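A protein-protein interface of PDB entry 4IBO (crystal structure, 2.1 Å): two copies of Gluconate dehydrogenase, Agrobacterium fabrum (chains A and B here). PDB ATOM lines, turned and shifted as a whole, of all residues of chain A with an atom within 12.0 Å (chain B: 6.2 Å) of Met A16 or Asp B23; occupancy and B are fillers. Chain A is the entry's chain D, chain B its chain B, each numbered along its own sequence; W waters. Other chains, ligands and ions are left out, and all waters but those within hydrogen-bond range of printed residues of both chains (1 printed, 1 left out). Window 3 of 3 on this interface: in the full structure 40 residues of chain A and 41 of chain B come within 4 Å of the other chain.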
ATOM      1  N   MET A  16       2.823 -18.583 -22.459  1.00  0.00           N
ATOM      2  CA  MET A  16       1.995 -19.135 -23.529  1.00  0.00           C
ATOM      3  C   MET A  16       0.799 -18.241 -23.855  1.00  0.00           C
ATOM      4  O   MET A  16       0.415 -18.110 -25.021  1.00  0.00           O
ATOM      5  CB  MET A  16       1.538 -20.562 -23.195  1.00  0.00           C
ATOM      6  CG  MET A  16       0.324 -21.018 -23.987  1.00  0.00           C
ATOM      7  SD  MET A  16       0.254 -22.794 -24.280  1.00  0.00           S
ATOM      8  CE  MET A  16      -1.416 -22.962 -24.918  1.00  0.00           C
ATOM      9  N   SER A  17       0.213 -17.624 -22.832  1.00  0.00           N
ATOM     10  CA  SER A  17      -0.884 -16.680 -23.056  1.00  0.00           C
ATOM     11  C   SER A  17      -0.427 -15.451 -23.830  1.00  0.00           C
ATOM     12  O   SER A  17       0.652 -14.905 -23.568  1.00  0.00           O
ATOM     13  CB  SER A  17      -1.503 -16.216 -21.739  1.00  0.00           C
ATOM     14  OG  SER A  17      -2.296 -15.060 -21.972  1.00  0.00           O
ATOM     15  N   ASN A  18      -1.260 -15.000 -24.761  1.00  0.00           N
ATOM     16  CA  ASN A  18      -0.958 -13.797 -25.529  1.00  0.00           C
ATOM     17  C   ASN A  18      -1.639 -12.526 -25.004  1.00  0.00           C
ATOM     18  O   ASN A  18      -1.678 -11.507 -25.699  1.00  0.00           O
ATOM     19  CB  ASN A  18      -1.304 -14.012 -27.006  1.00  0.00           C
ATOM     20  CG  ASN A  18      -2.791 -14.234 -27.232  1.00  0.00           C
ATOM     21  OD1 ASN A  18      -3.516 -14.659 -26.323  1.00  0.00           O
ATOM     22  ND2 ASN A  18      -3.254 -13.957 -28.452  1.00  0.00           N
ATOM     23  N   GLN A  19      -2.178 -12.578 -23.786  1.00  0.00           N
ATOM     24  CA  GLN A  19      -2.795 -11.392 -23.177  1.00  0.00           C
ATOM     25  C   GLN A  19      -1.830 -10.188 -23.160  1.00  0.00           C
ATOM     26  O   GLN A  19      -0.617 -10.371 -23.038  1.00  0.00           O
ATOM     27  CB  GLN A  19      -3.254 -11.717 -21.753  1.00  0.00           C
ATOM     28  CG  GLN A  19      -2.108 -11.972 -20.776  1.00  0.00           C
ATOM     29  CD  GLN A  19      -2.605 -12.398 -19.414  1.00  0.00           C
ATOM     30  OE1 GLN A  19      -3.745 -12.099 -19.045  1.00  0.00           O
ATOM     31  NE2 GLN A  19      -1.763 -13.117 -18.664  1.00  0.00           N
ATOM     32  N   ILE A  20      -2.375  -8.971 -23.269  1.00  0.00           N
ATOM     33  CA  ILE A  20      -1.574  -7.746 -23.411  1.00  0.00           C
ATOM     34  C   ILE A  20      -1.751  -6.707 -22.296  1.00  0.00           C
ATOM     35  O   ILE A  20      -1.044  -5.695 -22.267  1.00  0.00           O
ATOM     36  CB  ILE A  20      -1.900  -7.030 -24.741  1.00  0.00           C
ATOM     37  CG1 ILE A  20      -3.226  -6.262 -24.629  1.00  0.00           C
ATOM     38  CG2 ILE A  20      -1.915  -8.025 -25.898  1.00  0.00           C
ATOM     39  CD1 ILE A  20      -3.814  -5.841 -25.963  1.00  0.00           C
ATOM     40  N   ILE A  21      -2.685  -6.937 -21.379  1.00  0.00           N
ATOM     41  CA  ILE A  21      -3.007  -5.921 -20.366  1.00  0.00           C
ATOM     42  C   ILE A  21      -1.909  -5.725 -19.309  1.00  0.00           C
ATOM     43  O   ILE A  21      -1.983  -4.809 -18.485  1.00  0.00           O
ATOM     44  CB  ILE A  21      -4.344  -6.246 -19.667  1.00  0.00           C
ATOM     45  CG1 ILE A  21      -4.250  -7.601 -18.973  1.00  0.00           C
ATOM     46  CG2 ILE A  21      -5.494  -6.235 -20.690  1.00  0.00           C
ATOM     47  CD1 ILE A  21      -5.541  -8.054 -18.292  1.00  0.00           C
ATOM     48  N   PHE A  22      -0.900  -6.598 -19.314  1.00  0.00           N
ATOM     49  CA  PHE A  22       0.239  -6.440 -18.412  1.00  0.00           C
ATOM     50  C   PHE A  22       1.528  -5.962 -19.113  1.00  0.00           C
ATOM     51  O   PHE A  22       2.590  -5.912 -18.490  1.00  0.00           O
ATOM     52  CB  PHE A  22       0.494  -7.740 -17.650  1.00  0.00           C
ATOM     53  CG  PHE A  22      -0.684  -8.188 -16.822  1.00  0.00           C
ATOM     54  CD1 PHE A  22      -0.987  -7.554 -15.627  1.00  0.00           C
ATOM     55  CD2 PHE A  22      -1.501  -9.232 -17.253  1.00  0.00           C
ATOM     56  CE1 PHE A  22      -2.084  -7.963 -14.857  1.00  0.00           C
ATOM     57  CE2 PHE A  22      -2.604  -9.644 -16.490  1.00  0.00           C
ATOM     58  CZ  PHE A  22      -2.890  -9.009 -15.295  1.00  0.00           C
ATOM     59  N   ASP A  23       1.428  -5.608 -20.395  1.00  0.00           N
ATOM     60  CA  ASP A  23       2.599  -5.169 -21.161  1.00  0.00           C
ATOM     61  C   ASP A  23       2.911  -3.688 -20.937  1.00  0.00           C
ATOM     62  O   ASP A  23       2.005  -2.849 -20.957  1.00  0.00           O
ATOM     63  CB  ASP A  23       2.398  -5.440 -22.660  1.00  0.00           C
ATOM     64  CG  ASP A  23       3.473  -4.772 -23.531  1.00  0.00           C
ATOM     65  OD1 ASP A  23       4.638  -5.240 -23.537  1.00  0.00           O
ATOM     66  OD2 ASP A  23       3.156  -3.781 -24.225  1.00  0.00           O
ATOM     67  N   VAL A  48      11.277  -6.015 -17.513  1.00  0.00           N
ATOM     68  CA  VAL A  48      10.928  -7.306 -18.093  1.00  0.00           C
ATOM     69  C   VAL A  48       9.556  -7.230 -18.765  1.00  0.00           C
ATOM     70  O   VAL A  48       9.319  -7.870 -19.778  1.00  0.00           O
ATOM     71  CB  VAL A  48      10.979  -8.440 -17.051  1.00  0.00           C
ATOM     72  CG1 VAL A  48      10.391  -9.728 -17.627  1.00  0.00           C
ATOM     73  CG2 VAL A  48      12.418  -8.675 -16.603  1.00  0.00           C
ATOM     74  N   ALA A  49       8.672  -6.404 -18.217  1.00  0.00           N
ATOM     75  CA  ALA A  49       7.345  -6.218 -18.790  1.00  0.00           C
ATOM     76  C   ALA A  49       7.372  -5.259 -19.983  1.00  0.00           C
ATOM     77  O   ALA A  49       6.354  -5.067 -20.642  1.00  0.00           O
ATOM     78  CB  ALA A  49       6.369  -5.722 -17.717  1.00  0.00           C
ATOM     79  N   VAL A 242       7.142  -7.695  -7.776  1.00  0.00           N
ATOM     80  CA  VAL A 242       7.111  -7.402  -9.212  1.00  0.00           C
ATOM     81  C   VAL A 242       5.695  -7.434  -9.789  1.00  0.00           C
ATOM     82  O   VAL A 242       5.285  -6.499 -10.485  1.00  0.00           O
ATOM     83  CB  VAL A 242       8.018  -8.348  -9.993  1.00  0.00           C
ATOM     84  CG1 VAL A 242       7.805  -8.181 -11.488  1.00  0.00           C
ATOM     85  CG2 VAL A 242       9.478  -8.072  -9.637  1.00  0.00           C
ATOM     86  N   GLY A 243       4.952  -8.498  -9.487  1.00  0.00           N
ATOM     87  CA  GLY A 243       3.598  -8.662  -9.995  1.00  0.00           C
ATOM     88  C   GLY A 243       2.724  -7.464  -9.673  1.00  0.00           C
ATOM     89  O   GLY A 243       2.026  -6.947 -10.548  1.00  0.00           O
ATOM     90  N   THR A 244       2.776  -7.013  -8.422  1.00  0.00           N
ATOM     91  CA  THR A 244       1.973  -5.879  -7.986  1.00  0.00           C
ATOM     92  C   THR A 244       2.424  -4.589  -8.678  1.00  0.00           C
ATOM     93  O   THR A 244       1.601  -3.761  -9.070  1.00  0.00           O
ATOM     94  CB  THR A 244       2.039  -5.717  -6.453  1.00  0.00           C
ATOM     95  OG1 THR A 244       1.705  -6.969  -5.836  1.00  0.00           O
ATOM     96  CG2 THR A 244       1.053  -4.651  -5.960  1.00  0.00           C
ATOM     97  N   VAL A 246       3.977  -4.243 -11.604  1.00  0.00           N
ATOM     98  CA  VAL A 246       3.614  -4.294 -13.016  1.00  0.00           C
ATOM     99  C   VAL A 246       2.111  -4.077 -13.180  1.00  0.00           C
ATOM    100  O   VAL A 246       1.679  -3.295 -14.029  1.00  0.00           O
ATOM    101  CB  VAL A 246       4.012  -5.633 -13.661  1.00  0.00           C
ATOM    102  CG1 VAL A 246       3.334  -5.799 -15.044  1.00  0.00           C
ATOM    103  CG2 VAL A 246       5.533  -5.734 -13.789  1.00  0.00           C
ATOM    104  N   PHE A 247       1.324  -4.782 -12.371  1.00  0.00           N
ATOM    105  CA  PHE A 247      -0.127  -4.633 -12.378  1.00  0.00           C
ATOM    106  C   PHE A 247      -0.523  -3.160 -12.219  1.00  0.00           C
ATOM    107  O   PHE A 247      -1.324  -2.639 -13.007  1.00  0.00           O
ATOM    108  CB  PHE A 247      -0.731  -5.495 -11.271  1.00  0.00           C
ATOM    109  CG  PHE A 247      -2.158  -5.169 -10.933  1.00  0.00           C
ATOM    110  CD1 PHE A 247      -3.180  -5.395 -11.846  1.00  0.00           C
ATOM    111  CD2 PHE A 247      -2.485  -4.680  -9.675  1.00  0.00           C
ATOM    112  CE1 PHE A 247      -4.502  -5.112 -11.515  1.00  0.00           C
ATOM    113  CE2 PHE A 247      -3.805  -4.396  -9.339  1.00  0.00           C
ATOM    114  CZ  PHE A 247      -4.812  -4.611 -10.261  1.00  0.00           C
ATOM    115  N   ALA A 252      -3.904  -3.008 -16.979  1.00  0.00           N
ATOM    116  CA  ALA A 252      -4.653  -3.944 -16.151  1.00  0.00           C
ATOM    117  C   ALA A 252      -5.281  -3.252 -14.958  1.00  0.00           C
ATOM    118  O   ALA A 252      -6.233  -3.766 -14.375  1.00  0.00           O
ATOM    119  CB  ALA A 252      -3.745  -5.064 -15.672  1.00  0.00           C
ATOM    120  N   GLN B  19       4.937 -12.772 -20.273  1.00  0.00           N
ATOM    121  CA  GLN B  19       5.218 -12.744 -18.845  1.00  0.00           C
ATOM    122  C   GLN B  19       4.567 -13.925 -18.146  1.00  0.00           C
ATOM    123  O   GLN B  19       3.335 -13.970 -17.951  1.00  0.00           O
ATOM    124  CB  GLN B  19       4.723 -11.443 -18.216  1.00  0.00           C
ATOM    125  CG  GLN B  19       5.790 -10.367 -18.065  1.00  0.00           C
ATOM    126  CD  GLN B  19       5.213  -9.092 -17.479  1.00  0.00           C
ATOM    127  OE1 GLN B  19       5.570  -8.694 -16.368  1.00  0.00           O
ATOM    128  NE2 GLN B  19       4.301  -8.450 -18.223  1.00  0.00           N
ATOM    129  N   ILE B  20       5.405 -14.874 -17.744  1.00  0.00           N
ATOM    130  CA  ILE B  20       4.911 -16.081 -17.106  1.00  0.00           C
ATOM    131  C   ILE B  20       4.193 -15.787 -15.783  1.00  0.00           C
ATOM    132  O   ILE B  20       3.281 -16.519 -15.412  1.00  0.00           O
ATOM    133  CB  ILE B  20       6.040 -17.119 -16.894  1.00  0.00           C
ATOM    134  CG1 ILE B  20       6.992 -16.668 -15.786  1.00  0.00           C
ATOM    135  CG2 ILE B  20       6.798 -17.349 -18.197  1.00  0.00           C
ATOM    136  CD1 ILE B  20       8.152 -17.606 -15.571  1.00  0.00           C
ATOM    137  N   ILE B  21       4.571 -14.711 -15.085  1.00  0.00           N
ATOM    138  CA  ILE B  21       3.981 -14.457 -13.764  1.00  0.00           C
ATOM    139  C   ILE B  21       2.489 -14.126 -13.815  1.00  0.00           C
ATOM    140  O   ILE B  21       1.807 -14.184 -12.794  1.00  0.00           O
ATOM    141  CB  ILE B  21       4.721 -13.366 -12.944  1.00  0.00           C
ATOM    142  CG1 ILE B  21       4.628 -11.995 -13.625  1.00  0.00           C
ATOM    143  CG2 ILE B  21       6.188 -13.756 -12.696  1.00  0.00           C
ATOM    144  CD1 ILE B  21       5.161 -10.856 -12.736  1.00  0.00           C
ATOM    145  N   PHE B  22       1.981 -13.776 -14.993  1.00  0.00           N
ATOM    146  CA  PHE B  22       0.548 -13.543 -15.140  1.00  0.00           C
ATOM    147  C   PHE B  22      -0.131 -14.663 -15.913  1.00  0.00           C
ATOM    148  O   PHE B  22      -1.333 -14.617 -16.152  1.00  0.00           O
ATOM    149  CB  PHE B  22       0.278 -12.182 -15.795  1.00  0.00           C
ATOM    150  CG  PHE B  22       0.770 -11.026 -14.981  1.00  0.00           C
ATOM    151  CD1 PHE B  22       0.086 -10.625 -13.835  1.00  0.00           C
ATOM    152  CD2 PHE B  22       1.923 -10.353 -15.336  1.00  0.00           C
ATOM    153  CE1 PHE B  22       0.548  -9.566 -13.069  1.00  0.00           C
ATOM    154  CE2 PHE B  22       2.383  -9.279 -14.571  1.00  0.00           C
ATOM    155  CZ  PHE B  22       1.694  -8.894 -13.440  1.00  0.00           C
ATOM    156  N   ASP B  23       0.633 -15.680 -16.286  1.00  0.00           N
ATOM    157  CA  ASP B  23       0.081 -16.767 -17.092  1.00  0.00           C
ATOM    158  C   ASP B  23      -0.637 -17.804 -16.229  1.00  0.00           C
ATOM    159  O   ASP B  23      -0.126 -18.211 -15.185  1.00  0.00           O
ATOM    160  CB  ASP B  23       1.183 -17.459 -17.895  1.00  0.00           C
ATOM    161  CG  ASP B  23       0.625 -18.463 -18.897  1.00  0.00           C
ATOM    162  OD1 ASP B  23       0.416 -18.088 -20.064  1.00  0.00           O
ATOM    163  OD2 ASP B  23       0.380 -19.620 -18.521  1.00  0.00           O
ATOM    164  N   LEU B  24      -1.806 -18.253 -16.682  1.00  0.00           N
ATOM    165  CA  LEU B  24      -2.604 -19.197 -15.907  1.00  0.00           C
ATOM    166  C   LEU B  24      -2.689 -20.554 -16.590  1.00  0.00           C
ATOM    167  O   LEU B  24      -3.545 -21.370 -16.250  1.00  0.00           O
ATOM    168  CB  LEU B  24      -4.021 -18.659 -15.692  1.00  0.00           C
ATOM    169  CG  LEU B  24      -4.137 -17.312 -14.984  1.00  0.00           C
ATOM    170  CD1 LEU B  24      -5.595 -16.967 -14.737  1.00  0.00           C
ATOM    171  CD2 LEU B  24      -3.363 -17.359 -13.665  1.00  0.00           C
ATOM    172  N   GLY B  25      -1.819 -20.787 -17.568  1.00  0.00           N
ATOM    173  CA  GLY B  25      -1.801 -22.066 -18.263  1.00  0.00           C
ATOM    174  C   GLY B  25      -1.609 -23.209 -17.282  1.00  0.00           C
ATOM    175  O   GLY B  25      -0.766 -23.125 -16.386  1.00  0.00           O
ATOM    176  N   GLY B  26      -2.403 -24.267 -17.431  1.00  0.00           N
ATOM    177  CA  GLY B  26      -2.273 -25.431 -16.569  1.00  0.00           C
ATOM    178  C   GLY B  26      -3.092 -25.299 -15.296  1.00  0.00           C
ATOM    179  O   GLY B  26      -3.144 -26.225 -14.487  1.00  0.00           O
ATOM    180  N   ARG B  27      -3.736 -24.149 -15.115  1.00  0.00           N
ATOM    181  CA  ARG B  27      -4.603 -23.938 -13.960  1.00  0.00           C
ATOM    182  C   ARG B  27      -6.072 -24.034 -14.370  1.00  0.00           C
ATOM    183  O   ARG B  27      -6.427 -23.722 -15.511  1.00  0.00           O
ATOM    184  CB  ARG B  27      -4.300 -22.579 -13.303  1.00  0.00           C
ATOM    185  CG  ARG B  27      -2.910 -22.514 -12.662  1.00  0.00           C
ATOM    186  CD  ARG B  27      -2.809 -23.587 -11.595  1.00  0.00           C
ATOM    187  NE  ARG B  27      -1.440 -23.968 -11.252  1.00  0.00           N
ATOM    188  CZ  ARG B  27      -0.989 -25.220 -11.298  1.00  0.00           C
ATOM    189  NH1 ARG B  27      -1.797 -26.208 -11.677  1.00  0.00           N
ATOM    190  NH2 ARG B  27       0.266 -25.488 -10.964  1.00  0.00           N
ATOM    191  N   ALA B  49      -6.012 -15.529 -20.171  1.00  0.00           N
ATOM    192  CA  ALA B  49      -4.721 -15.656 -19.474  1.00  0.00           C
ATOM    193  C   ALA B  49      -4.250 -17.110 -19.420  1.00  0.00           C
ATOM    194  O   ALA B  49      -3.154 -17.393 -18.927  1.00  0.00           O
ATOM    195  CB  ALA B  49      -4.821 -15.069 -18.054  1.00  0.00           C
ATOM    196  N   GLY B  50      -5.087 -18.030 -19.904  1.00  0.00           N
ATOM    197  CA  GLY B  50      -4.691 -19.423 -20.046  1.00  0.00           C
ATOM    198  C   GLY B  50      -5.440 -20.458 -19.209  1.00  0.00           C
ATOM    199  O   GLY B  50      -5.236 -21.652 -19.390  1.00  0.00           O
ATOM    200  N   VAL B 246      -6.993 -11.640 -12.898  1.00  0.00           N
ATOM    201  CA  VAL B 246      -5.828 -12.413 -13.344  1.00  0.00           C
ATOM    202  C   VAL B 246      -4.659 -12.293 -12.351  1.00  0.00           C
ATOM    203  O   VAL B 246      -4.062 -13.305 -11.959  1.00  0.00           O
ATOM    204  CB  VAL B 246      -5.401 -12.034 -14.775  1.00  0.00           C
ATOM    205  CG1 VAL B 246      -4.111 -12.757 -15.168  1.00  0.00           C
ATOM    206  CG2 VAL B 246      -6.511 -12.391 -15.769  1.00  0.00           C
ATOM    207  N   SER B 249      -5.103 -14.383  -9.387  1.00  0.00           N
ATOM    208  CA  SER B 249      -5.170 -15.817  -9.685  1.00  0.00           C
ATOM    209  C   SER B 249      -3.812 -16.398 -10.090  1.00  0.00           C
ATOM    210  O   SER B 249      -3.664 -17.616 -10.225  1.00  0.00           O
ATOM    211  CB  SER B 249      -6.170 -16.077 -10.821  1.00  0.00           C
ATOM    212  OG  SER B 249      -7.459 -15.609 -10.469  1.00  0.00           O
ATOM    213  N   ALA B 250      -2.830 -15.524 -10.279  1.00  0.00           N
ATOM    214  CA  ALA B 250      -1.558 -15.897 -10.886  1.00  0.00           C
ATOM    215  C   ALA B 250      -0.420 -15.871  -9.864  1.00  0.00           C
ATOM    216  O   ALA B 250      -0.591 -15.392  -8.741  1.00  0.00           O
ATOM    217  CB  ALA B 250      -1.248 -14.959 -12.066  1.00  0.00           C
ATOM    218  N   SER B 251       0.752 -16.364 -10.259  1.00  0.00           N
ATOM    219  CA  SER B 251       1.904 -16.373  -9.345  1.00  0.00           C
ATOM    220  C   SER B 251       2.346 -14.959  -8.961  1.00  0.00           C
ATOM    221  O   SER B 251       2.999 -14.762  -7.936  1.00  0.00           O
ATOM    222  CB  SER B 251       3.070 -17.141  -9.956  1.00  0.00           C
ATOM    223  OG  SER B 251       3.645 -16.397 -11.012  1.00  0.00           O
HETATM  224  O   HOH W   1       0.819 -13.829 -19.574  1.00  0.00           O
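O of Phe A22 sits at hydrogen-bond distance from NE2 of Gln B19, at 3.1 Å.
O of Phe B22 lies within hydrogen-bond range of NE2 of Gln A19, 3.0 Å away.
The backbone NH (N) of Met A16 sits at hydrogen-bond distance from the side-chain carboxylate (OD1) of Asp B23 (3.4 Å).
The side-chain carboxylate (OD1) of Asp B23 sits at hydrogen-bond distance from the backbone NH (N) of Ser A17 (2.8 Å).
Water W1 lies within hydrogen-bond range of the side-chain amide nitrogen of Gln A19 and the backbone carbonyl oxygen of Gln B19.
Among the printed residues, merely in contact across the chains: Gln A19 with Ala B49 (3.3 Å), Ala A49 with Gln B19 (3.4 Å), Ser A17 with Ala B49 (3.5 Å), Gly A243 with Phe B22 (3.5 Å), Phe A22 with Phe B22 (3.6 Å), Val A246 with Phe B22 (3.6 Å), Phe A22 with Val B246 (3.7 Å), Gly A243 with Ile B21 (3.8 Å), Val A246 with Gln B19 (3.9 Å), Gln A19 with Val B246 (3.9 Å) and Val A242 with Ile B21 (3.96 Å).
The side-chain hydroxyl of Ser B251 lies close to the backbone carbonyl oxygen of Ile B21 (3.4 Å).
OD2 of Asp B23 lies within hydrogen-bond range of N of Gly B25.
The backbone NH (N) of Leu B24 lies within hydrogen-bond range of the backbone carbonyl oxygen (O) of Ala B49, at 2.8 Å.
The side-chain hydroxyl (OG) of Ser A17 is in hydrogen-bond range of the backbone NH (N) of Gln A19 (3.1 Å).
Gln A19 touches Phe B22, and with the chains exchanged Phe A22 touches Gln B19.
Gln A19 touches Val B246, and with the chains exchanged Val A246 touches Gln B19.
Phe B22 touches its own counterpart, Phe A22.
Phe A22 touches Val B246, and with the chains exchanged Val A246 touches Phe B22.
7 positions are printed for both chains.
Met A16 touches just one residue of chain B: Asp B23 (3.4 Å).
Printed residues of chain B within 4 Å of Ser A17: Asp B23 and Ala B49.
Of the printed residues of chain B, Ala A49 touches Gln B19.
Printed residues of chain B within 4 Å of Gly A243: Ile B21 (3.8 Å) and Phe B22 (3.5 Å).
Of the printed residues of chain B, Val A246 touches Gln B19 and Phe B22.
Phe A247 touches none of the printed residues of chain B.
No residue of chain A comes within 4 Å of Ile B20.
Of chain A, only Met A16 (3.4 Å) and Ser A17 (2.8 Å) come within 4 Å of Asp B23.
Gly B26 touches none of the printed residues of chain A.
No residue of chain A comes within 4 Å of Gly B50.
Printed residues of chain A within 4 Å of Val B246: Gln A19 and Phe A22.
No residue of chain A comes within 4 Å of Ala B250.
The nearest residue of chain B that does not touch Met A16 is Ile B20 (6.0 Å).
Hydrophobic or aromatic side chains of chain A that line the printed part of chain B: Phe A22, Ala A49, Val A242 and Val A246.
Of the 15 printed residues of chain B, 6 touch a printed residue of chain A.
Among the printed residues, 15 pairs touch across the chains.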
